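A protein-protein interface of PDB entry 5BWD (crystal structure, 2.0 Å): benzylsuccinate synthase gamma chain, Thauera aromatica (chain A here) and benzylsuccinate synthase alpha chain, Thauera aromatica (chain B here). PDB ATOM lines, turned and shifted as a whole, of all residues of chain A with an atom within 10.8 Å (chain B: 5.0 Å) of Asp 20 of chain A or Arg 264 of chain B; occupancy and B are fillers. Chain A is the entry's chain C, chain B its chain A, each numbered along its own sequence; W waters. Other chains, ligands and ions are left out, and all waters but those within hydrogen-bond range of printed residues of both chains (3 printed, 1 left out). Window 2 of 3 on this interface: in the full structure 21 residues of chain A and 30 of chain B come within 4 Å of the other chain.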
ATOM      1  N   PRO A  14       7.954   2.366   7.435  1.00  0.00           N
ATOM      2  CA  PRO A  14       6.680   2.262   6.712  1.00  0.00           C
ATOM      3  C   PRO A  14       6.756   1.345   5.497  1.00  0.00           C
ATOM      4  O   PRO A  14       7.632   1.515   4.648  1.00  0.00           O
ATOM      5  CB  PRO A  14       6.408   3.705   6.284  1.00  0.00           C
ATOM      6  CG  PRO A  14       7.062   4.524   7.341  1.00  0.00           C
ATOM      7  CD  PRO A  14       8.303   3.768   7.729  1.00  0.00           C
ATOM      8  N   VAL A  15       5.848   0.377   5.429  1.00  0.00           N
ATOM      9  CA  VAL A  15       5.817  -0.561   4.318  1.00  0.00           C
ATOM     10  C   VAL A  15       5.479   0.183   3.035  1.00  0.00           C
ATOM     11  O   VAL A  15       4.495   0.920   2.985  1.00  0.00           O
ATOM     12  CB  VAL A  15       4.811  -1.697   4.574  1.00  0.00           C
ATOM     13  CG1 VAL A  15       4.820  -2.685   3.419  1.00  0.00           C
ATOM     14  CG2 VAL A  15       5.130  -2.403   5.885  1.00  0.00           C
ATOM     15  N   PRO A  16       6.311   0.010   1.997  1.00  0.00           N
ATOM     16  CA  PRO A  16       6.067   0.620   0.686  1.00  0.00           C
ATOM     17  C   PRO A  16       4.695   0.245   0.130  1.00  0.00           C
ATOM     18  O   PRO A  16       4.239  -0.881   0.327  1.00  0.00           O
ATOM     19  CB  PRO A  16       7.191   0.044  -0.180  1.00  0.00           C
ATOM     20  CG  PRO A  16       8.279  -0.270   0.785  1.00  0.00           C
ATOM     21  CD  PRO A  16       7.583  -0.732   2.031  1.00  0.00           C
ATOM     22  N   LYS A  17       4.050   1.183  -0.556  1.00  0.00           N
ATOM     23  CA  LYS A  17       2.682   0.984  -1.021  1.00  0.00           C
ATOM     24  C   LYS A  17       2.590  -0.009  -2.176  1.00  0.00           C
ATOM     25  O   LYS A  17       1.493  -0.373  -2.604  1.00  0.00           O
ATOM     26  CB  LYS A  17       2.066   2.323  -1.433  1.00  0.00           C
ATOM     27  CG  LYS A  17       2.111   3.381  -0.339  1.00  0.00           C
ATOM     28  CD  LYS A  17       1.200   4.558  -0.655  1.00  0.00           C
ATOM     29  CE  LYS A  17      -0.257   4.124  -0.717  1.00  0.00           C
ATOM     30  NZ  LYS A  17      -1.187   5.280  -0.844  1.00  0.00           N
ATOM     31  N   ASP A  18       3.740  -0.450  -2.678  1.00  0.00           N
ATOM     32  CA  ASP A  18       3.765  -1.420  -3.768  1.00  0.00           C
ATOM     33  C   ASP A  18       4.160  -2.807  -3.267  1.00  0.00           C
ATOM     34  O   ASP A  18       4.350  -3.730  -4.058  1.00  0.00           O
ATOM     35  CB  ASP A  18       4.724  -0.964  -4.872  1.00  0.00           C
ATOM     36  CG  ASP A  18       6.161  -0.878  -4.400  1.00  0.00           C
ATOM     37  OD1 ASP A  18       6.381  -0.699  -3.184  1.00  0.00           O
ATOM     38  OD2 ASP A  18       7.074  -0.985  -5.246  1.00  0.00           O
ATOM     39  N   ALA A  19       4.279  -2.949  -1.950  1.00  0.00           N
ATOM     40  CA  ALA A  19       4.633  -4.232  -1.353  1.00  0.00           C
ATOM     41  C   ALA A  19       3.424  -5.162  -1.302  1.00  0.00           C
ATOM     42  O   ALA A  19       2.284  -4.707  -1.212  1.00  0.00           O
ATOM     43  CB  ALA A  19       5.204  -4.029   0.036  1.00  0.00           C
ATOM     44  N   ASP A  20       3.684  -6.466  -1.356  1.00  0.00           N
ATOM     45  CA  ASP A  20       2.627  -7.472  -1.332  1.00  0.00           C
ATOM     46  C   ASP A  20       1.837  -7.430  -0.029  1.00  0.00           C
ATOM     47  O   ASP A  20       0.649  -7.742  -0.004  1.00  0.00           O
ATOM     48  CB  ASP A  20       3.215  -8.871  -1.528  1.00  0.00           C
ATOM     49  CG  ASP A  20       3.889  -9.038  -2.875  1.00  0.00           C
ATOM     50  OD1 ASP A  20       4.072  -8.025  -3.579  1.00  0.00           O
ATOM     51  OD2 ASP A  20       4.241 -10.184  -3.225  1.00  0.00           O
ATOM     52  N   ASP A  21       2.510  -7.047   1.049  1.00  0.00           N
ATOM     53  CA  ASP A  21       1.912  -7.065   2.377  1.00  0.00           C
ATOM     54  C   ASP A  21       1.484  -5.676   2.830  1.00  0.00           C
ATOM     55  O   ASP A  21       1.261  -5.453   4.020  1.00  0.00           O
ATOM     56  CB  ASP A  21       2.897  -7.646   3.393  1.00  0.00           C
ATOM     57  CG  ASP A  21       4.171  -6.827   3.500  1.00  0.00           C
ATOM     58  OD1 ASP A  21       4.814  -6.587   2.455  1.00  0.00           O
ATOM     59  OD2 ASP A  21       4.524  -6.410   4.624  1.00  0.00           O
ATOM     60  N   TYR A  22       1.373  -4.739   1.894  1.00  0.00           N
ATOM     61  CA  TYR A  22       1.071  -3.363   2.266  1.00  0.00           C
ATOM     62  C   TYR A  22      -0.348  -3.198   2.802  1.00  0.00           C
ATOM     63  O   TYR A  22      -1.309  -3.720   2.236  1.00  0.00           O
ATOM     64  CB  TYR A  22       1.272  -2.408   1.086  1.00  0.00           C
ATOM     65  CG  TYR A  22       0.799  -1.004   1.397  1.00  0.00           C
ATOM     66  CD1 TYR A  22       1.552  -0.161   2.205  1.00  0.00           C
ATOM     67  CD2 TYR A  22      -0.410  -0.528   0.903  1.00  0.00           C
ATOM     68  CE1 TYR A  22       1.121   1.118   2.504  1.00  0.00           C
ATOM     69  CE2 TYR A  22      -0.850   0.751   1.198  1.00  0.00           C
ATOM     70  CZ  TYR A  22      -0.081   1.570   1.998  1.00  0.00           C
ATOM     71  OH  TYR A  22      -0.511   2.844   2.295  1.00  0.00           O
ATOM     72  N   GLU A  23      -0.454  -2.467   3.907  1.00  0.00           N
ATOM     73  CA  GLU A  23      -1.734  -2.015   4.442  1.00  0.00           C
ATOM     74  C   GLU A  23      -1.555  -0.586   4.935  1.00  0.00           C
ATOM     75  O   GLU A  23      -0.439  -0.174   5.253  1.00  0.00           O
ATOM     76  CB  GLU A  23      -2.220  -2.914   5.581  1.00  0.00           C
ATOM     77  CG  GLU A  23      -2.542  -4.343   5.178  1.00  0.00           C
ATOM     78  CD  GLU A  23      -3.149  -5.141   6.315  1.00  0.00           C
ATOM     79  OE1 GLU A  23      -4.162  -4.686   6.888  1.00  0.00           O
ATOM     80  OE2 GLU A  23      -2.609  -6.220   6.642  1.00  0.00           O
ATOM     81  N   ALA A  24      -2.647   0.168   4.995  1.00  0.00           N
ATOM     82  CA  ALA A  24      -2.594   1.543   5.480  1.00  0.00           C
ATOM     83  C   ALA A  24      -2.014   1.596   6.892  1.00  0.00           C
ATOM     84  O   ALA A  24      -2.540   0.974   7.813  1.00  0.00           O
ATOM     85  CB  ALA A  24      -3.980   2.175   5.448  1.00  0.00           C
ATOM     86  N   LYS A  26       0.780   0.369   8.000  1.00  0.00           N
ATOM     87  CA  LYS A  26       1.649  -0.744   8.368  1.00  0.00           C
ATOM     88  C   LYS A  26       3.118  -0.355   8.230  1.00  0.00           C
ATOM     89  O   LYS A  26       3.495   0.374   7.312  1.00  0.00           O
ATOM     90  CB  LYS A  26       1.351  -1.982   7.514  1.00  0.00           C
ATOM     91  CG  LYS A  26       2.199  -3.197   7.884  1.00  0.00           C
ATOM     92  CD  LYS A  26       1.905  -4.402   7.005  1.00  0.00           C
ATOM     93  CE  LYS A  26       0.596  -5.062   7.389  1.00  0.00           C
ATOM     94  NZ  LYS A  26       0.328  -6.276   6.570  1.00  0.00           N
ATOM     95  N   ASP A  28       7.424  -1.867   9.290  1.00  0.00           N
ATOM     96  CA  ASP A  28       8.332  -2.842   9.880  1.00  0.00           C
ATOM     97  C   ASP A  28       9.010  -2.231  11.099  1.00  0.00           C
ATOM     98  O   ASP A  28       9.679  -1.204  10.987  1.00  0.00           O
ATOM     99  CB  ASP A  28       9.399  -3.294   8.874  1.00  0.00           C
ATOM    100  CG  ASP A  28       8.817  -4.035   7.687  1.00  0.00           C
ATOM    101  OD1 ASP A  28       7.850  -4.802   7.870  1.00  0.00           O
ATOM    102  OD2 ASP A  28       9.339  -3.853   6.567  1.00  0.00           O
ATOM    103  N   SER A  43      12.548  -8.053  12.607  1.00  0.00           N
ATOM    104  CA  SER A  43      11.557  -7.243  11.905  1.00  0.00           C
ATOM    105  C   SER A  43      10.143  -7.702  12.239  1.00  0.00           C
ATOM    106  O   SER A  43       9.717  -8.779  11.829  1.00  0.00           O
ATOM    107  CB  SER A  43      11.784  -7.307  10.393  1.00  0.00           C
ATOM    108  OG  SER A  43      10.797  -6.567   9.697  1.00  0.00           O
ATOM    109  N   PRO A  45       6.017  -6.779  12.132  1.00  0.00           N
ATOM    110  CA  PRO A  45       4.958  -5.978  11.509  1.00  0.00           C
ATOM    111  C   PRO A  45       4.109  -5.261  12.551  1.00  0.00           C
ATOM    112  O   PRO A  45       3.591  -5.920  13.451  1.00  0.00           O
ATOM    113  CB  PRO A  45       4.115  -7.018  10.755  1.00  0.00           C
ATOM    114  CG  PRO A  45       4.934  -8.268  10.735  1.00  0.00           C
ATOM    115  CD  PRO A  45       5.785  -8.220  11.959  1.00  0.00           C
ATOM    116  N   LEU B 212       4.685 -18.031  -8.235  1.00  0.00           N
ATOM    117  CA  LEU B 212       3.740 -17.275  -9.050  1.00  0.00           C
ATOM    118  C   LEU B 212       3.083 -18.179 -10.091  1.00  0.00           C
ATOM    119  O   LEU B 212       1.885 -18.079 -10.342  1.00  0.00           O
ATOM    120  CB  LEU B 212       4.436 -16.097  -9.735  1.00  0.00           C
ATOM    121  CG  LEU B 212       4.768 -14.902  -8.841  1.00  0.00           C
ATOM    122  CD1 LEU B 212       5.653 -13.906  -9.580  1.00  0.00           C
ATOM    123  CD2 LEU B 212       3.492 -14.227  -8.357  1.00  0.00           C
ATOM    124  N   VAL B 259       3.626 -17.145   1.232  1.00  0.00           N
ATOM    125  CA  VAL B 259       5.035 -17.521   1.243  1.00  0.00           C
ATOM    126  C   VAL B 259       5.834 -16.477   0.475  1.00  0.00           C
ATOM    127  O   VAL B 259       6.911 -16.071   0.910  1.00  0.00           O
ATOM    128  CB  VAL B 259       5.265 -18.934   0.661  1.00  0.00           C
ATOM    129  CG1 VAL B 259       6.756 -19.186   0.458  1.00  0.00           C
ATOM    130  CG2 VAL B 259       4.676 -19.991   1.575  1.00  0.00           C
ATOM    131  N   ILE B 260       5.303 -16.038  -0.664  1.00  0.00           N
ATOM    132  CA  ILE B 260       5.957 -15.003  -1.461  1.00  0.00           C
ATOM    133  C   ILE B 260       6.091 -13.718  -0.651  1.00  0.00           C
ATOM    134  O   ILE B 260       7.163 -13.110  -0.613  1.00  0.00           O
ATOM    135  CB  ILE B 260       5.202 -14.735  -2.778  1.00  0.00           C
ATOM    136  CG1 ILE B 260       5.268 -15.958  -3.697  1.00  0.00           C
ATOM    137  CG2 ILE B 260       5.794 -13.528  -3.488  1.00  0.00           C
ATOM    138  CD1 ILE B 260       4.487 -15.789  -4.992  1.00  0.00           C
ATOM    139  N   SER B 261       5.002 -13.309  -0.004  1.00  0.00           N
ATOM    140  CA  SER B 261       5.005 -12.092   0.808  1.00  0.00           C
ATOM    141  C   SER B 261       6.032 -12.178   1.938  1.00  0.00           C
ATOM    142  O   SER B 261       6.753 -11.223   2.217  1.00  0.00           O
ATOM    143  CB  SER B 261       3.611 -11.834   1.387  1.00  0.00           C
ATOM    144  OG  SER B 261       3.610 -10.655   2.170  1.00  0.00           O
ATOM    145  N   TRP B 262       6.085 -13.344   2.572  1.00  0.00           N
ATOM    146  CA  TRP B 262       7.013 -13.640   3.660  1.00  0.00           C
ATOM    147  C   TRP B 262       8.472 -13.553   3.200  1.00  0.00           C
ATOM    148  O   TRP B 262       9.314 -12.924   3.856  1.00  0.00           O
ATOM    149  CB  TRP B 262       6.672 -15.030   4.204  1.00  0.00           C
ATOM    150  CG  TRP B 262       7.589 -15.650   5.209  1.00  0.00           C
ATOM    151  CD1 TRP B 262       7.750 -15.289   6.514  1.00  0.00           C
ATOM    152  CD2 TRP B 262       8.404 -16.812   5.010  1.00  0.00           C
ATOM    153  NE1 TRP B 262       8.644 -16.134   7.132  1.00  0.00           N
ATOM    154  CE2 TRP B 262       9.058 -17.077   6.228  1.00  0.00           C
ATOM    155  CE3 TRP B 262       8.655 -17.643   3.914  1.00  0.00           C
ATOM    156  CZ2 TRP B 262       9.949 -18.137   6.379  1.00  0.00           C
ATOM    157  CZ3 TRP B 262       9.540 -18.696   4.067  1.00  0.00           C
ATOM    158  CH2 TRP B 262      10.176 -18.933   5.290  1.00  0.00           C
ATOM    159  N   ALA B 263       8.760 -14.166   2.057  1.00  0.00           N
ATOM    160  CA  ALA B 263      10.105 -14.143   1.492  1.00  0.00           C
ATOM    161  C   ALA B 263      10.532 -12.718   1.155  1.00  0.00           C
ATOM    162  O   ALA B 263      11.668 -12.320   1.409  1.00  0.00           O
ATOM    163  CB  ALA B 263      10.170 -15.021   0.255  1.00  0.00           C
ATOM    164  N   ARG B 264       9.611 -11.951   0.586  1.00  0.00           N
ATOM    165  CA  ARG B 264       9.904 -10.583   0.185  1.00  0.00           C
ATOM    166  C   ARG B 264      10.038  -9.651   1.385  1.00  0.00           C
ATOM    167  O   ARG B 264      10.808  -8.691   1.344  1.00  0.00           O
ATOM    168  CB  ARG B 264       8.829 -10.079  -0.780  1.00  0.00           C
ATOM    169  CG  ARG B 264       8.947 -10.723  -2.152  1.00  0.00           C
ATOM    170  CD  ARG B 264       7.821 -10.336  -3.094  1.00  0.00           C
ATOM    171  NE  ARG B 264       8.139 -10.737  -4.463  1.00  0.00           N
ATOM    172  CZ  ARG B 264       7.260 -10.768  -5.459  1.00  0.00           C
ATOM    173  NH1 ARG B 264       7.647 -11.145  -6.673  1.00  0.00           N
ATOM    174  NH2 ARG B 264       5.996 -10.429  -5.241  1.00  0.00           N
ATOM    175  N   ARG B 265       9.306  -9.937   2.457  1.00  0.00           N
ATOM    176  CA  ARG B 265       9.440  -9.149   3.679  1.00  0.00           C
ATOM    177  C   ARG B 265      10.793  -9.445   4.326  1.00  0.00           C
ATOM    178  O   ARG B 265      11.405  -8.568   4.938  1.00  0.00           O
ATOM    179  CB  ARG B 265       8.289  -9.438   4.649  1.00  0.00           C
ATOM    180  CG  ARG B 265       8.244  -8.502   5.854  1.00  0.00           C
ATOM    181  CD  ARG B 265       6.874  -8.507   6.532  1.00  0.00           C
ATOM    182  NE  ARG B 265       6.492  -9.834   7.000  1.00  0.00           N
ATOM    183  CZ  ARG B 265       6.781 -10.311   8.206  1.00  0.00           C
ATOM    184  NH1 ARG B 265       6.396 -11.532   8.550  1.00  0.00           N
ATOM    185  NH2 ARG B 265       7.460  -9.565   9.068  1.00  0.00           N
ATOM    186  N   GLN B 266      11.254 -10.684   4.174  1.00  0.00           N
ATOM    187  CA  GLN B 266      12.596 -11.077   4.603  1.00  0.00           C
ATOM    188  C   GLN B 266      13.648 -10.296   3.827  1.00  0.00           C
ATOM    189  O   GLN B 266      14.647  -9.846   4.387  1.00  0.00           O
ATOM    190  CB  GLN B 266      12.811 -12.581   4.407  1.00  0.00           C
ATOM    191  CG  GLN B 266      14.200 -13.072   4.804  1.00  0.00           C
ATOM    192  CD  GLN B 266      14.368 -13.208   6.304  1.00  0.00           C
ATOM    193  OE1 GLN B 266      13.494 -13.735   6.993  1.00  0.00           O
ATOM    194  NE2 GLN B 266      15.496 -12.729   6.821  1.00  0.00           N
ATOM    195  N   GLY B 267      13.417 -10.140   2.527  1.00  0.00           N
ATOM    196  CA  GLY B 267      14.305  -9.361   1.687  1.00  0.00           C
ATOM    197  C   GLY B 267      14.305  -7.899   2.079  1.00  0.00           C
ATOM    198  O   GLY B 267      15.337  -7.229   2.026  1.00  0.00           O
ATOM    199  N   ARG B 268      13.138  -7.405   2.481  1.00  0.00           N
ATOM    200  CA  ARG B 268      13.010  -6.019   2.910  1.00  0.00           C
ATOM    201  C   ARG B 268      13.834  -5.779   4.170  1.00  0.00           C
ATOM    202  O   ARG B 268      14.446  -4.724   4.326  1.00  0.00           O
ATOM    203  CB  ARG B 268      11.541  -5.663   3.147  1.00  0.00           C
ATOM    204  CG  ARG B 268      11.279  -4.172   3.272  1.00  0.00           C
ATOM    205  CD  ARG B 268       9.804  -3.856   3.090  1.00  0.00           C
ATOM    206  NE  ARG B 268       8.987  -4.424   4.159  1.00  0.00           N
ATOM    207  CZ  ARG B 268       7.866  -5.107   3.964  1.00  0.00           C
ATOM    208  NH1 ARG B 268       7.190  -5.582   5.001  1.00  0.00           N
ATOM    209  NH2 ARG B 268       7.417  -5.317   2.733  1.00  0.00           N
ATOM    210  N   CYS B 294      15.769 -12.678  -2.358  1.00  0.00           N
ATOM    211  CA  CYS B 294      14.520 -12.897  -1.637  1.00  0.00           C
ATOM    212  C   CYS B 294      13.324 -12.283  -2.360  1.00  0.00           C
ATOM    213  O   CYS B 294      12.212 -12.806  -2.290  1.00  0.00           O
ATOM    214  CB  CYS B 294      14.622 -12.333  -0.220  1.00  0.00           C
ATOM    215  SG  CYS B 294      15.728 -13.271   0.847  1.00  0.00           S
ATOM    216  N   GLN B 295      13.556 -11.174  -3.053  1.00  0.00           N
ATOM    217  CA  GLN B 295      12.495 -10.511  -3.800  1.00  0.00           C
ATOM    218  C   GLN B 295      12.000 -11.391  -4.948  1.00  0.00           C
ATOM    219  O   GLN B 295      10.796 -11.516  -5.169  1.00  0.00           O
ATOM    220  CB  GLN B 295      12.980  -9.161  -4.337  1.00  0.00           C
ATOM    221  CG  GLN B 295      11.928  -8.380  -5.111  1.00  0.00           C
ATOM    222  CD  GLN B 295      10.774  -7.924  -4.233  1.00  0.00           C
ATOM    223  OE1 GLN B 295      10.925  -7.760  -3.023  1.00  0.00           O
ATOM    224  NE2 GLN B 295       9.609  -7.722  -4.843  1.00  0.00           N
ATOM    225  N   ALA B 299       9.217 -16.522  -5.590  1.00  0.00           N
ATOM    226  CA  ALA B 299       8.154 -16.067  -6.482  1.00  0.00           C
ATOM    227  C   ALA B 299       8.428 -16.503  -7.919  1.00  0.00           C
ATOM    228  O   ALA B 299       7.526 -16.959  -8.626  1.00  0.00           O
ATOM    229  CB  ALA B 299       8.008 -14.559  -6.411  1.00  0.00           C
ATOM    230  N   GLU B 300       9.682 -16.367  -8.336  1.00  0.00           N
ATOM    231  CA  GLU B 300      10.096 -16.675  -9.703  1.00  0.00           C
ATOM    232  C   GLU B 300      10.914 -17.965  -9.737  1.00  0.00           C
ATOM    233  O   GLU B 300      11.356 -18.444  -8.689  1.00  0.00           O
ATOM    234  CB  GLU B 300      10.915 -15.512 -10.280  1.00  0.00           C
ATOM    235  CG  GLU B 300      10.228 -14.155 -10.202  1.00  0.00           C
ATOM    236  CD  GLU B 300      11.138 -13.015 -10.631  1.00  0.00           C
ATOM    237  OE1 GLU B 300      10.730 -11.842 -10.496  1.00  0.00           O
ATOM    238  OE2 GLU B 300      12.262 -13.290 -11.102  1.00  0.00           O
HETATM  239  O   HOH W   1       9.437  -1.457   5.529  1.00  0.00           O
HETATM  240  O   HOH W   2      11.005  -6.252   6.771  1.00  0.00           O
HETATM  241  O   HOH W   3       8.150  -6.822   9.458  1.00  0.00           O
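The side-chain carboxylate (OD2) of Asp 20 of chain A is in salt-bridge range of the guanidinium group (NH2) of Arg 264 of chain B (2.7 Å).
The guanidinium group (NH1) of Arg 268 of chain B is in salt-bridge range of the side-chain carboxylate (OD2) of Asp 21 of chain A (2.8 Å).
The guanidinium group of Arg 268 of chain B lies within salt-bridge range of the side-chain carboxylate of Asp 28 of chain A (2.5 Å).
NE of Arg 264 of chain B lies within hydrogen-bond range of O of Gln 295 of chain B (2.9 Å).
The backbone NH of Val 15 of chain A is in hydrogen-bond range of the backbone carbonyl oxygen of Lys 26 of chain A.
The side-chain amino group (NZ) of Lys 26 of chain A is in hydrogen-bond range of the backbone carbonyl oxygen (O) of Asp 21 of chain A.
Val 15 of chain A touches Arg 268 of chain B.
Arg 268 of chain B touches Pro 16 of chain A (CD to CD, 3.98 Å).
NH2 of Arg 268 of chain B touches CB of Ala 19 of chain A, 3.7 Å away.
Asp 20 of chain A touches Ile 260 of chain B.
Asp 21 of chain A touches Ser 261 of chain B (CB to OG, 3.3 Å).
CD of Arg 265 of chain B touches OD2 of Asp 21 of chain A, 3.7 Å away.
Ser 43 of chain A touches Arg 265 of chain B (O to NH2, 3.7 Å).
Pro 45 of chain A touches Arg 265 of chain B (CG to NH2, 3.3 Å).
Of chain B, only Ile 260 (3.7 Å) and Arg 264 (2.7 Å) come within 4 Å of Asp 20 of chain A.
Of chain A, only Asp 20 (2.7 Å) comes within 4 Å of Arg 264 of chain B.
Of chain A, only Asp 20 comes within 4 Å of Ile 260 of chain B.
Ser 261 of chain B touches just one residue of chain A: Asp 21 (3.3 Å).
Ala 263 of chain B touches none of the printed residues of chain A.
Printed residues of chain A within 4 Å of Arg 268 of chain B: Val 15 (3.8 Å), Pro 16 (3.98 Å), Ala 19 (3.7 Å), Asp 21 (2.8 Å) and Asp 28 (2.5 Å).
No residue of chain A comes within 4 Å of Cys 294 of chain B.
No residue of chain A comes within 4 Å of Gln 295 of chain B.
Ala 299 of chain B touches none of the printed residues of chain A.
Printed residues of chain B within 4 Å of Pro 16 of chain A: Arg 268 (3.98 Å).
Printed residues of chain B within 4 Å of Asp 28 of chain A: Arg 268.
The nearest residue of chain B that does not touch Asp 20 of chain A is Ser 261 of chain B (4.1 Å).
The nearest residue of chain A that does not touch Arg 264 of chain B is Asp 21 of chain A (6.2 Å).
The nearest printed residue of chain B that does not touch Asp 28 of chain A is Arg 265 of chain B (4.1 Å).
Of the 15 printed residues of chain B, 5 touch a printed residue of chain A.
Printed residues of chain B that touch a printed residue of chain A: Ile 260, Ser 261, Arg 264, Arg 265 and Arg 268.
Hydrophobic or aromatic side chains of chain B within 4 Å of the printed part of chain A: Ile 260.
Among the printed residues, Asp or Glu carboxylates within 4 Å of a Lys or Arg side-chain nitrogen of the other chain: Asp 20 of chain A with Arg 264 of chain B (2.7 Å), Asp 21 of chain A with Arg 268 of chain B (2.8 Å) and Asp 28 of chain A with Arg 268 of chain B (2.5 Å).
Water W3 lies within hydrogen-bond range of the side-chain carboxylate of Asp 28 of chain A (2.6 Å), the side-chain hydroxyl of Ser 43 of chain A (2.7 Å) and the guanidinium group of Arg 265 of chain B (2.9 Å).
Water W1 bridges OD2 of Asp 28 of chain A and NE of Arg 268 of chain B.
Water W2 lies within hydrogen-bond range of OD2 of Asp 28 of chain A (2.9 Å), OG of Ser 43 of chain A (3.0 Å) and O of Arg 265 of chain B (3.0 Å).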
